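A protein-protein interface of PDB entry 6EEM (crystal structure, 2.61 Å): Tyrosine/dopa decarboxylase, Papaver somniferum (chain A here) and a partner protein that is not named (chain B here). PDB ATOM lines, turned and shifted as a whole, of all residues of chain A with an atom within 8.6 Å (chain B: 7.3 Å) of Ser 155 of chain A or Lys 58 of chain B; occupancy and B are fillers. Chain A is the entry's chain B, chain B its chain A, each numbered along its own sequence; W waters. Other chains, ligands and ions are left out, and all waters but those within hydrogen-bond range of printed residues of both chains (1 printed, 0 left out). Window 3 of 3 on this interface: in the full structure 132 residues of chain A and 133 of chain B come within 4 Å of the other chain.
Water W1 bridges N of Lys 58 of chain B (2.9 Å) and OE1 of Glu 132 of chain A (2.9 Å).
Of the printed residues of chain B, Ala 129 of chain A touches Tyr 56 (3.6 Å). Of the printed residues of chain B, Leu 133 of chain A touches Leu 57 (3.6 Å) and Leu 61 (3.6 Å). Printed residues of chain B within 4 Å of Trp 140 of chain A: Pro 62 (3.0 Å) and Glu 63 (3.5 Å). Ser 155 of chain A touches just one residue of chain B: Lys 58. Printed residues of chain A within 4 Å of Tyr 56 of chain B: Ala 129 and Glu 132. Lys 58 of chain B touches three residues of chain A. Of the printed residues of chain A, Pro 62 of chain B touches Trp 140 (3.0 Å). The nearest residue of chain A that does not touch Lys 58 of chain B is Asp 156 of chain A (5.8 Å).
The backbone NH (N) of Gly 55 of chain B sits at hydrogen-bond distance from the side-chain carboxylate (OE2) of Glu 132 of chain A, 2.7 Å away. The side-chain carboxylate of Glu 132 of chain A sits at hydrogen-bond distance from the backbone NH of Tyr 56 of chain B, 3.2 Å away. The side-chain carboxylate (OE1) of Glu 132 of chain A sits at hydrogen-bond distance from the backbone NH (N) of Leu 57 of chain B, at 2.8 Å. O of Pro 62 of chain B sits at hydrogen-bond distance from NE1 of Trp 140 of chain A, at 3.0 Å. OE1 of Gln 143 of chain A sits close to O of Glu 63 of chain B.
Among the printed residues, pairs that only touch across the chains: Ser 155 of chain A with Lys 58 of chain B, Trp 140 of chain A with Glu 63 of chain B, Leu 133 of chain A with Leu 57 of chain B, Leu 133 of chain A with Leu 61 of chain B, Ile 136 of chain A with Leu 57 of chain B, Ala 129 of chain A with Tyr 56 of chain B, Ile 136 of chain A with Lys 58 of chain B and Glu 132 of chain A with Lys 58 of chain B.
Of the 18 printed residues of chain A, 7 touch a printed residue of chain B. Printed residues of chain A that touch a printed residue of chain B: Ala 129, Glu 132, Leu 133, Ile 136, Trp 140, Gln 143 and Ser 155. Hydrophobic or aromatic side chains of chain A that line the printed part of chain B: Ala 129, Leu 133, Ile 136 and Trp 140. Along chain A the printed residues that touch a printed residue of chain B span positions 129 to 155. Of the 9 printed residues of chain B, 7 touch a printed residue of chain A. Hydrophobic or aromatic side chains of chain B within 4 Å of the printed part of chain A: Tyr 56, Leu 57 and Leu 61. Among the printed residues, no Asp or Glu carboxylate lies within 4 Å of a Lys or Arg side-chain nitrogen of the other chain.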
ATOM      1  N   PRO A 128       1.793 -13.511  13.647  1.00  0.00           N
ATOM      2  CA  PRO A 128       2.215 -14.369  14.766  1.00  0.00           C
ATOM      3  C   PRO A 128       3.099 -13.642  15.766  1.00  0.00           C
ATOM      4  O   PRO A 128       2.990 -13.879  16.978  1.00  0.00           O
ATOM      5  CB  PRO A 128       2.960 -15.513  14.059  1.00  0.00           C
ATOM      6  CG  PRO A 128       2.388 -15.547  12.680  1.00  0.00           C
ATOM      7  CD  PRO A 128       2.067 -14.125  12.333  1.00  0.00           C
ATOM      8  N   ALA A 129       3.959 -12.742  15.284  1.00  0.00           N
ATOM      9  CA  ALA A 129       4.927 -12.089  16.160  1.00  0.00           C
ATOM     10  C   ALA A 129       4.232 -11.247  17.226  1.00  0.00           C
ATOM     11  O   ALA A 129       4.598 -11.299  18.399  1.00  0.00           O
ATOM     12  CB  ALA A 129       5.889 -11.241  15.330  1.00  0.00           C
ATOM     13  N   GLU A 132       2.872 -13.748  19.921  1.00  0.00           N
ATOM     14  CA  GLU A 132       3.882 -14.510  20.646  1.00  0.00           C
ATOM     15  C   GLU A 132       4.795 -13.600  21.461  1.00  0.00           C
ATOM     16  O   GLU A 132       5.138 -13.923  22.606  1.00  0.00           O
ATOM     17  CB  GLU A 132       4.683 -15.380  19.678  1.00  0.00           C
ATOM     18  CG  GLU A 132       3.856 -16.523  19.110  1.00  0.00           C
ATOM     19  CD  GLU A 132       4.671 -17.562  18.364  1.00  0.00           C
ATOM     20  OE1 GLU A 132       5.901 -17.670  18.589  1.00  0.00           O
ATOM     21  OE2 GLU A 132       4.061 -18.278  17.546  1.00  0.00           O
ATOM     22  N   LEU A 133       5.204 -12.462  20.895  1.00  0.00           N
ATOM     23  CA  LEU A 133       6.003 -11.519  21.661  1.00  0.00           C
ATOM     24  C   LEU A 133       5.236 -11.021  22.872  1.00  0.00           C
ATOM     25  O   LEU A 133       5.810 -10.882  23.956  1.00  0.00           O
ATOM     26  CB  LEU A 133       6.444 -10.342  20.791  1.00  0.00           C
ATOM     27  CG  LEU A 133       7.496  -9.459  21.479  1.00  0.00           C
ATOM     28  CD1 LEU A 133       8.739 -10.255  21.808  1.00  0.00           C
ATOM     29  CD2 LEU A 133       7.857  -8.238  20.654  1.00  0.00           C
ATOM     30  N   SER A 135       3.006 -12.609  24.612  1.00  0.00           N
ATOM     31  CA  SER A 135       3.056 -13.670  25.618  1.00  0.00           C
ATOM     32  C   SER A 135       4.415 -13.715  26.307  1.00  0.00           C
ATOM     33  O   SER A 135       4.506 -13.714  27.545  1.00  0.00           O
ATOM     34  CB  SER A 135       2.739 -15.016  24.970  1.00  0.00           C
ATOM     35  OG  SER A 135       1.383 -15.076  24.570  1.00  0.00           O
ATOM     36  N   ILE A 136       5.487 -13.761  25.513  1.00  0.00           N
ATOM     37  CA  ILE A 136       6.839 -13.812  26.067  1.00  0.00           C
ATOM     38  C   ILE A 136       7.071 -12.643  27.018  1.00  0.00           C
ATOM     39  O   ILE A 136       7.526 -12.818  28.152  1.00  0.00           O
ATOM     40  CB  ILE A 136       7.880 -13.810  24.932  1.00  0.00           C
ATOM     41  CG1 ILE A 136       7.777 -15.086  24.086  1.00  0.00           C
ATOM     42  CG2 ILE A 136       9.287 -13.591  25.494  1.00  0.00           C
ATOM     43  CD1 ILE A 136       8.401 -14.949  22.719  1.00  0.00           C
ATOM     44  N   ASN A 139       5.277 -12.608  30.263  1.00  0.00           N
ATOM     45  CA  ASN A 139       5.960 -13.522  31.176  1.00  0.00           C
ATOM     46  C   ASN A 139       7.214 -12.876  31.759  1.00  0.00           C
ATOM     47  O   ASN A 139       7.473 -12.965  32.964  1.00  0.00           O
ATOM     48  CB  ASN A 139       6.298 -14.829  30.468  1.00  0.00           C
ATOM     49  CG  ASN A 139       5.392 -15.962  30.901  1.00  0.00           C
ATOM     50  OD1 ASN A 139       4.180 -15.777  31.048  1.00  0.00           O
ATOM     51  ND2 ASN A 139       5.976 -17.140  31.134  1.00  0.00           N
ATOM     52  N   TRP A 140       8.014 -12.233  30.909  1.00  0.00           N
ATOM     53  CA  TRP A 140       9.180 -11.492  31.381  1.00  0.00           C
ATOM     54  C   TRP A 140       8.815 -10.616  32.570  1.00  0.00           C
ATOM     55  O   TRP A 140       9.311 -10.809  33.689  1.00  0.00           O
ATOM     56  CB  TRP A 140       9.750 -10.621  30.256  1.00  0.00           C
ATOM     57  CG  TRP A 140      10.624 -11.327  29.254  1.00  0.00           C
ATOM     58  CD1 TRP A 140      10.735 -12.675  29.052  1.00  0.00           C
ATOM     59  CD2 TRP A 140      11.513 -10.707  28.319  1.00  0.00           C
ATOM     60  NE1 TRP A 140      11.633 -12.928  28.044  1.00  0.00           N
ATOM     61  CE2 TRP A 140      12.127 -11.737  27.579  1.00  0.00           C
ATOM     62  CE3 TRP A 140      11.842  -9.380  28.030  1.00  0.00           C
ATOM     63  CZ2 TRP A 140      13.059 -11.482  26.573  1.00  0.00           C
ATOM     64  CZ3 TRP A 140      12.767  -9.127  27.035  1.00  0.00           C
ATOM     65  CH2 TRP A 140      13.365 -10.175  26.315  1.00  0.00           C
ATOM     66  N   GLN A 143       7.548 -12.190  35.751  1.00  0.00           N
ATOM     67  CA  GLN A 143       8.630 -12.806  36.505  1.00  0.00           C
ATOM     68  C   GLN A 143       9.435 -11.746  37.251  1.00  0.00           C
ATOM     69  O   GLN A 143       9.781 -11.933  38.422  1.00  0.00           O
ATOM     70  CB  GLN A 143       9.515 -13.633  35.569  1.00  0.00           C
ATOM     71  CG  GLN A 143       8.849 -14.939  35.123  1.00  0.00           C
ATOM     72  CD  GLN A 143       9.441 -15.531  33.848  1.00  0.00           C
ATOM     73  OE1 GLN A 143      10.385 -14.991  33.264  1.00  0.00           O
ATOM     74  NE2 GLN A 143       8.881 -16.650  33.412  1.00  0.00           N
ATOM     75  N   LYS A 149       3.263 -18.261  39.860  1.00  0.00           N
ATOM     76  CA  LYS A 149       3.192 -18.919  38.558  1.00  0.00           C
ATOM     77  C   LYS A 149       1.753 -19.056  38.077  1.00  0.00           C
ATOM     78  O   LYS A 149       1.502 -19.078  36.868  1.00  0.00           O
ATOM     79  CB  LYS A 149       3.869 -20.290  38.611  1.00  0.00           C
ATOM     80  CG  LYS A 149       5.394 -20.247  38.561  1.00  0.00           C
ATOM     81  CD  LYS A 149       5.992 -21.620  38.869  1.00  0.00           C
ATOM     82  CE  LYS A 149       7.451 -21.716  38.434  1.00  0.00           C
ATOM     83  NZ  LYS A 149       7.606 -21.621  36.949  1.00  0.00           N
ATOM     84  N   LEU A 152       1.183 -16.539  35.358  1.00  0.00           N
ATOM     85  CA  LEU A 152       1.989 -16.463  34.152  1.00  0.00           C
ATOM     86  C   LEU A 152       1.570 -17.545  33.160  1.00  0.00           C
ATOM     87  O   LEU A 152       0.751 -18.420  33.459  1.00  0.00           O
ATOM     88  CB  LEU A 152       3.476 -16.581  34.499  1.00  0.00           C
ATOM     89  CG  LEU A 152       3.992 -15.586  35.545  1.00  0.00           C
ATOM     90  CD1 LEU A 152       5.506 -15.650  35.647  1.00  0.00           C
ATOM     91  CD2 LEU A 152       3.534 -14.160  35.258  1.00  0.00           C
ATOM     92  N   PHE A 153       2.133 -17.455  31.954  1.00  0.00           N
ATOM     93  CA  PHE A 153       1.932 -18.472  30.927  1.00  0.00           C
ATOM     94  C   PHE A 153       2.809 -19.670  31.255  1.00  0.00           C
ATOM     95  O   PHE A 153       4.039 -19.561  31.256  1.00  0.00           O
ATOM     96  CB  PHE A 153       2.260 -17.923  29.540  1.00  0.00           C
ATOM     97  CG  PHE A 153       1.175 -17.059  28.956  1.00  0.00           C
ATOM     98  CD1 PHE A 153       0.006 -17.630  28.468  1.00  0.00           C
ATOM     99  CD2 PHE A 153       1.319 -15.679  28.902  1.00  0.00           C
ATOM    100  CE1 PHE A 153      -0.996 -16.840  27.939  1.00  0.00           C
ATOM    101  CE2 PHE A 153       0.317 -14.882  28.372  1.00  0.00           C
ATOM    102  CZ  PHE A 153      -0.838 -15.463  27.888  1.00  0.00           C
ATOM    103  N   SER A 154       2.179 -20.805  31.550  1.00  0.00           N
ATOM    104  CA  SER A 154       2.906 -22.051  31.760  1.00  0.00           C
ATOM    105  C   SER A 154       3.333 -22.610  30.411  1.00  0.00           C
ATOM    106  O   SER A 154       2.491 -22.809  29.530  1.00  0.00           O
ATOM    107  CB  SER A 154       2.039 -23.058  32.511  1.00  0.00           C
ATOM    108  OG  SER A 154       0.703 -23.044  32.031  1.00  0.00           O
ATOM    109  N   SER A 155       4.635 -22.846  30.241  1.00  0.00           N
ATOM    110  CA  SER A 155       5.095 -23.493  29.014  1.00  0.00           C
ATOM    111  C   SER A 155       4.440 -24.857  28.828  1.00  0.00           C
ATOM    112  O   SER A 155       4.183 -25.274  27.693  1.00  0.00           O
ATOM    113  CB  SER A 155       6.621 -23.619  29.017  1.00  0.00           C
ATOM    114  OG  SER A 155       7.104 -24.015  30.288  1.00  0.00           O
ATOM    115  N   ASP A 156       4.148 -25.554  29.930  1.00  0.00           N
ATOM    116  CA  ASP A 156       3.439 -26.833  29.894  1.00  0.00           C
ATOM    117  C   ASP A 156       1.933 -26.608  29.727  1.00  0.00           C
ATOM    118  O   ASP A 156       1.108 -27.015  30.545  1.00  0.00           O
ATOM    119  CB  ASP A 156       3.746 -27.643  31.150  1.00  0.00           C
ATOM    120  CG  ASP A 156       3.490 -26.862  32.434  1.00  0.00           C
ATOM    121  OD1 ASP A 156       2.309 -26.634  32.777  1.00  0.00           O
ATOM    122  OD2 ASP A 156       4.474 -26.482  33.105  1.00  0.00           O
ATOM    123  N   GLY A 157       1.584 -25.938  28.632  1.00  0.00           N
ATOM    124  CA  GLY A 157       0.197 -25.643  28.333  1.00  0.00           C
ATOM    125  C   GLY A 157      -0.021 -24.286  27.695  1.00  0.00           C
ATOM    126  O   GLY A 157      -0.925 -24.115  26.878  1.00  0.00           O
ATOM    127  N   GLY A 161      -3.028 -19.815  33.695  1.00  0.00           N
ATOM    128  CA  GLY A 161      -2.870 -18.388  33.866  1.00  0.00           C
ATOM    129  C   GLY A 161      -2.442 -17.719  32.574  1.00  0.00           C
ATOM    130  O   GLY A 161      -2.374 -18.335  31.510  1.00  0.00           O
ATOM    131  N   GLN A 360      -4.387 -24.449  19.507  1.00  0.00           N
ATOM    132  CA  GLN A 360      -3.787 -24.057  20.785  1.00  0.00           C
ATOM    133  C   GLN A 360      -3.022 -22.739  20.680  1.00  0.00           C
ATOM    134  O   GLN A 360      -2.106 -22.471  21.463  1.00  0.00           O
ATOM    135  CB  GLN A 360      -2.878 -25.159  21.340  1.00  0.00           C
ATOM    136  CG  GLN A 360      -2.416 -24.910  22.771  1.00  0.00           C
ATOM    137  CD  GLN A 360      -1.710 -26.105  23.381  1.00  0.00           C
ATOM    138  OE1 GLN A 360      -1.881 -27.237  22.930  1.00  0.00           O
ATOM    139  NE2 GLN A 360      -0.912 -25.859  24.414  1.00  0.00           N
ATOM    140  N   GLY B  55       4.397 -20.976  17.952  1.00  0.00           N
ATOM    141  CA  GLY B  55       5.440 -21.204  18.929  1.00  0.00           C
ATOM    142  C   GLY B  55       6.844 -20.957  18.430  1.00  0.00           C
ATOM    143  O   GLY B  55       7.804 -21.310  19.127  1.00  0.00           O
ATOM    144  N   TYR B  56       6.996 -20.353  17.248  1.00  0.00           N
ATOM    145  CA  TYR B  56       8.322 -20.174  16.670  1.00  0.00           C
ATOM    146  C   TYR B  56       9.175 -19.229  17.509  1.00  0.00           C
ATOM    147  O   TYR B  56      10.380 -19.456  17.670  1.00  0.00           O
ATOM    148  CB  TYR B  56       8.201 -19.659  15.233  1.00  0.00           C
ATOM    149  CG  TYR B  56       8.193 -18.149  15.125  1.00  0.00           C
ATOM    150  CD1 TYR B  56       7.030 -17.419  15.341  1.00  0.00           C
ATOM    151  CD2 TYR B  56       9.354 -17.451  14.832  1.00  0.00           C
ATOM    152  CE1 TYR B  56       7.023 -16.046  15.260  1.00  0.00           C
ATOM    153  CE2 TYR B  56       9.356 -16.076  14.750  1.00  0.00           C
ATOM    154  CZ  TYR B  56       8.191 -15.377  14.967  1.00  0.00           C
ATOM    155  OH  TYR B  56       8.200 -14.003  14.886  1.00  0.00           O
ATOM    156  N   LEU B  57       8.565 -18.173  18.067  1.00  0.00           N
ATOM    157  CA  LEU B  57       9.351 -17.065  18.603  1.00  0.00           C
ATOM    158  C   LEU B  57       9.908 -17.372  19.987  1.00  0.00           C
ATOM    159  O   LEU B  57      11.065 -17.043  20.278  1.00  0.00           O
ATOM    160  CB  LEU B  57       8.515 -15.783  18.635  1.00  0.00           C
ATOM    161  CG  LEU B  57       9.225 -14.550  19.224  1.00  0.00           C
ATOM    162  CD1 LEU B  57      10.460 -14.167  18.419  1.00  0.00           C
ATOM    163  CD2 LEU B  57       8.280 -13.359  19.355  1.00  0.00           C
ATOM    164  N   LYS B  58       9.106 -17.987  20.857  1.00  0.00           N
ATOM    165  CA  LYS B  58       9.617 -18.398  22.161  1.00  0.00           C
ATOM    166  C   LYS B  58      10.942 -19.150  22.032  1.00  0.00           C
ATOM    167  O   LYS B  58      11.864 -18.941  22.825  1.00  0.00           O
ATOM    168  CB  LYS B  58       8.574 -19.256  22.882  1.00  0.00           C
ATOM    169  CG  LYS B  58       9.163 -20.249  23.853  1.00  0.00           C
ATOM    170  CD  LYS B  58       8.086 -21.089  24.532  1.00  0.00           C
ATOM    171  CE  LYS B  58       8.726 -22.121  25.473  1.00  0.00           C
ATOM    172  NZ  LYS B  58       7.729 -22.817  26.336  1.00  0.00           N
ATOM    173  N   LYS B  59      11.062 -20.024  21.029  1.00  0.00           N
ATOM    174  CA  LYS B  59      12.308 -20.765  20.867  1.00  0.00           C
ATOM    175  C   LYS B  59      13.497 -19.834  20.654  1.00  0.00           C
ATOM    176  O   LYS B  59      14.631 -20.189  20.994  1.00  0.00           O
ATOM    177  CB  LYS B  59      12.206 -21.741  19.695  1.00  0.00           C
ATOM    178  CG  LYS B  59      11.111 -22.793  19.798  1.00  0.00           C
ATOM    179  CD  LYS B  59      11.423 -23.940  18.841  1.00  0.00           C
ATOM    180  CE  LYS B  59      10.165 -24.568  18.257  1.00  0.00           C
ATOM    181  NZ  LYS B  59      10.496 -25.563  17.188  1.00  0.00           N
ATOM    182  N   ARG B  60      13.266 -18.648  20.094  1.00  0.00           N
ATOM    183  CA  ARG B  60      14.364 -17.794  19.661  1.00  0.00           C
ATOM    184  C   ARG B  60      14.767 -16.743  20.683  1.00  0.00           C
ATOM    185  O   ARG B  60      15.924 -16.304  20.674  1.00  0.00           O
ATOM    186  CB  ARG B  60      13.998 -17.082  18.361  1.00  0.00           C
ATOM    187  CG  ARG B  60      13.500 -17.982  17.269  1.00  0.00           C
ATOM    188  CD  ARG B  60      13.625 -17.260  15.954  1.00  0.00           C
ATOM    189  NE  ARG B  60      13.059 -17.998  14.835  1.00  0.00           N
ATOM    190  CZ  ARG B  60      13.342 -17.730  13.568  1.00  0.00           C
ATOM    191  NH1 ARG B  60      14.198 -16.755  13.282  1.00  0.00           N
ATOM    192  NH2 ARG B  60      12.784 -18.434  12.588  1.00  0.00           N
ATOM    193  N   LEU B  61      13.841 -16.307  21.545  1.00  0.00           N
ATOM    194  CA  LEU B  61      14.140 -15.262  22.511  1.00  0.00           C
ATOM    195  C   LEU B  61      14.406 -15.851  23.889  1.00  0.00           C
ATOM    196  O   LEU B  61      13.961 -16.959  24.208  1.00  0.00           O
ATOM    197  CB  LEU B  61      12.982 -14.265  22.598  1.00  0.00           C
ATOM    198  CG  LEU B  61      12.522 -13.616  21.295  1.00  0.00           C
ATOM    199  CD1 LEU B  61      11.559 -12.479  21.600  1.00  0.00           C
ATOM    200  CD2 LEU B  61      13.710 -13.129  20.484  1.00  0.00           C
ATOM    201  N   PRO B  62      15.133 -15.129  24.740  1.00  0.00           N
ATOM    202  CA  PRO B  62      15.345 -15.603  26.111  1.00  0.00           C
ATOM    203  C   PRO B  62      14.020 -15.721  26.846  1.00  0.00           C
ATOM    204  O   PRO B  62      13.010 -15.124  26.469  1.00  0.00           O
ATOM    205  CB  PRO B  62      16.233 -14.520  26.733  1.00  0.00           C
ATOM    206  CG  PRO B  62      16.840 -13.795  25.565  1.00  0.00           C
ATOM    207  CD  PRO B  62      15.795 -13.838  24.492  1.00  0.00           C
ATOM    208  N   GLU B  63      14.027 -16.511  27.913  1.00  0.00           N
ATOM    209  CA  GLU B  63      12.808 -16.729  28.679  1.00  0.00           C
ATOM    210  C   GLU B  63      12.661 -15.773  29.853  1.00  0.00           C
ATOM    211  O   GLU B  63      11.613 -15.774  30.506  1.00  0.00           O
ATOM    212  CB  GLU B  63      12.742 -18.180  29.172  1.00  0.00           C
ATOM    213  CG  GLU B  63      11.728 -19.023  28.402  1.00  0.00           C
ATOM    214  CD  GLU B  63      11.782 -20.491  28.770  1.00  0.00           C
ATOM    215  OE1 GLU B  63      10.955 -21.264  28.245  1.00  0.00           O
ATOM    216  OE2 GLU B  63      12.654 -20.868  29.583  1.00  0.00           O
HETATM  217  O   HOH W   1       6.277 -18.420  21.408  1.00  0.00           O
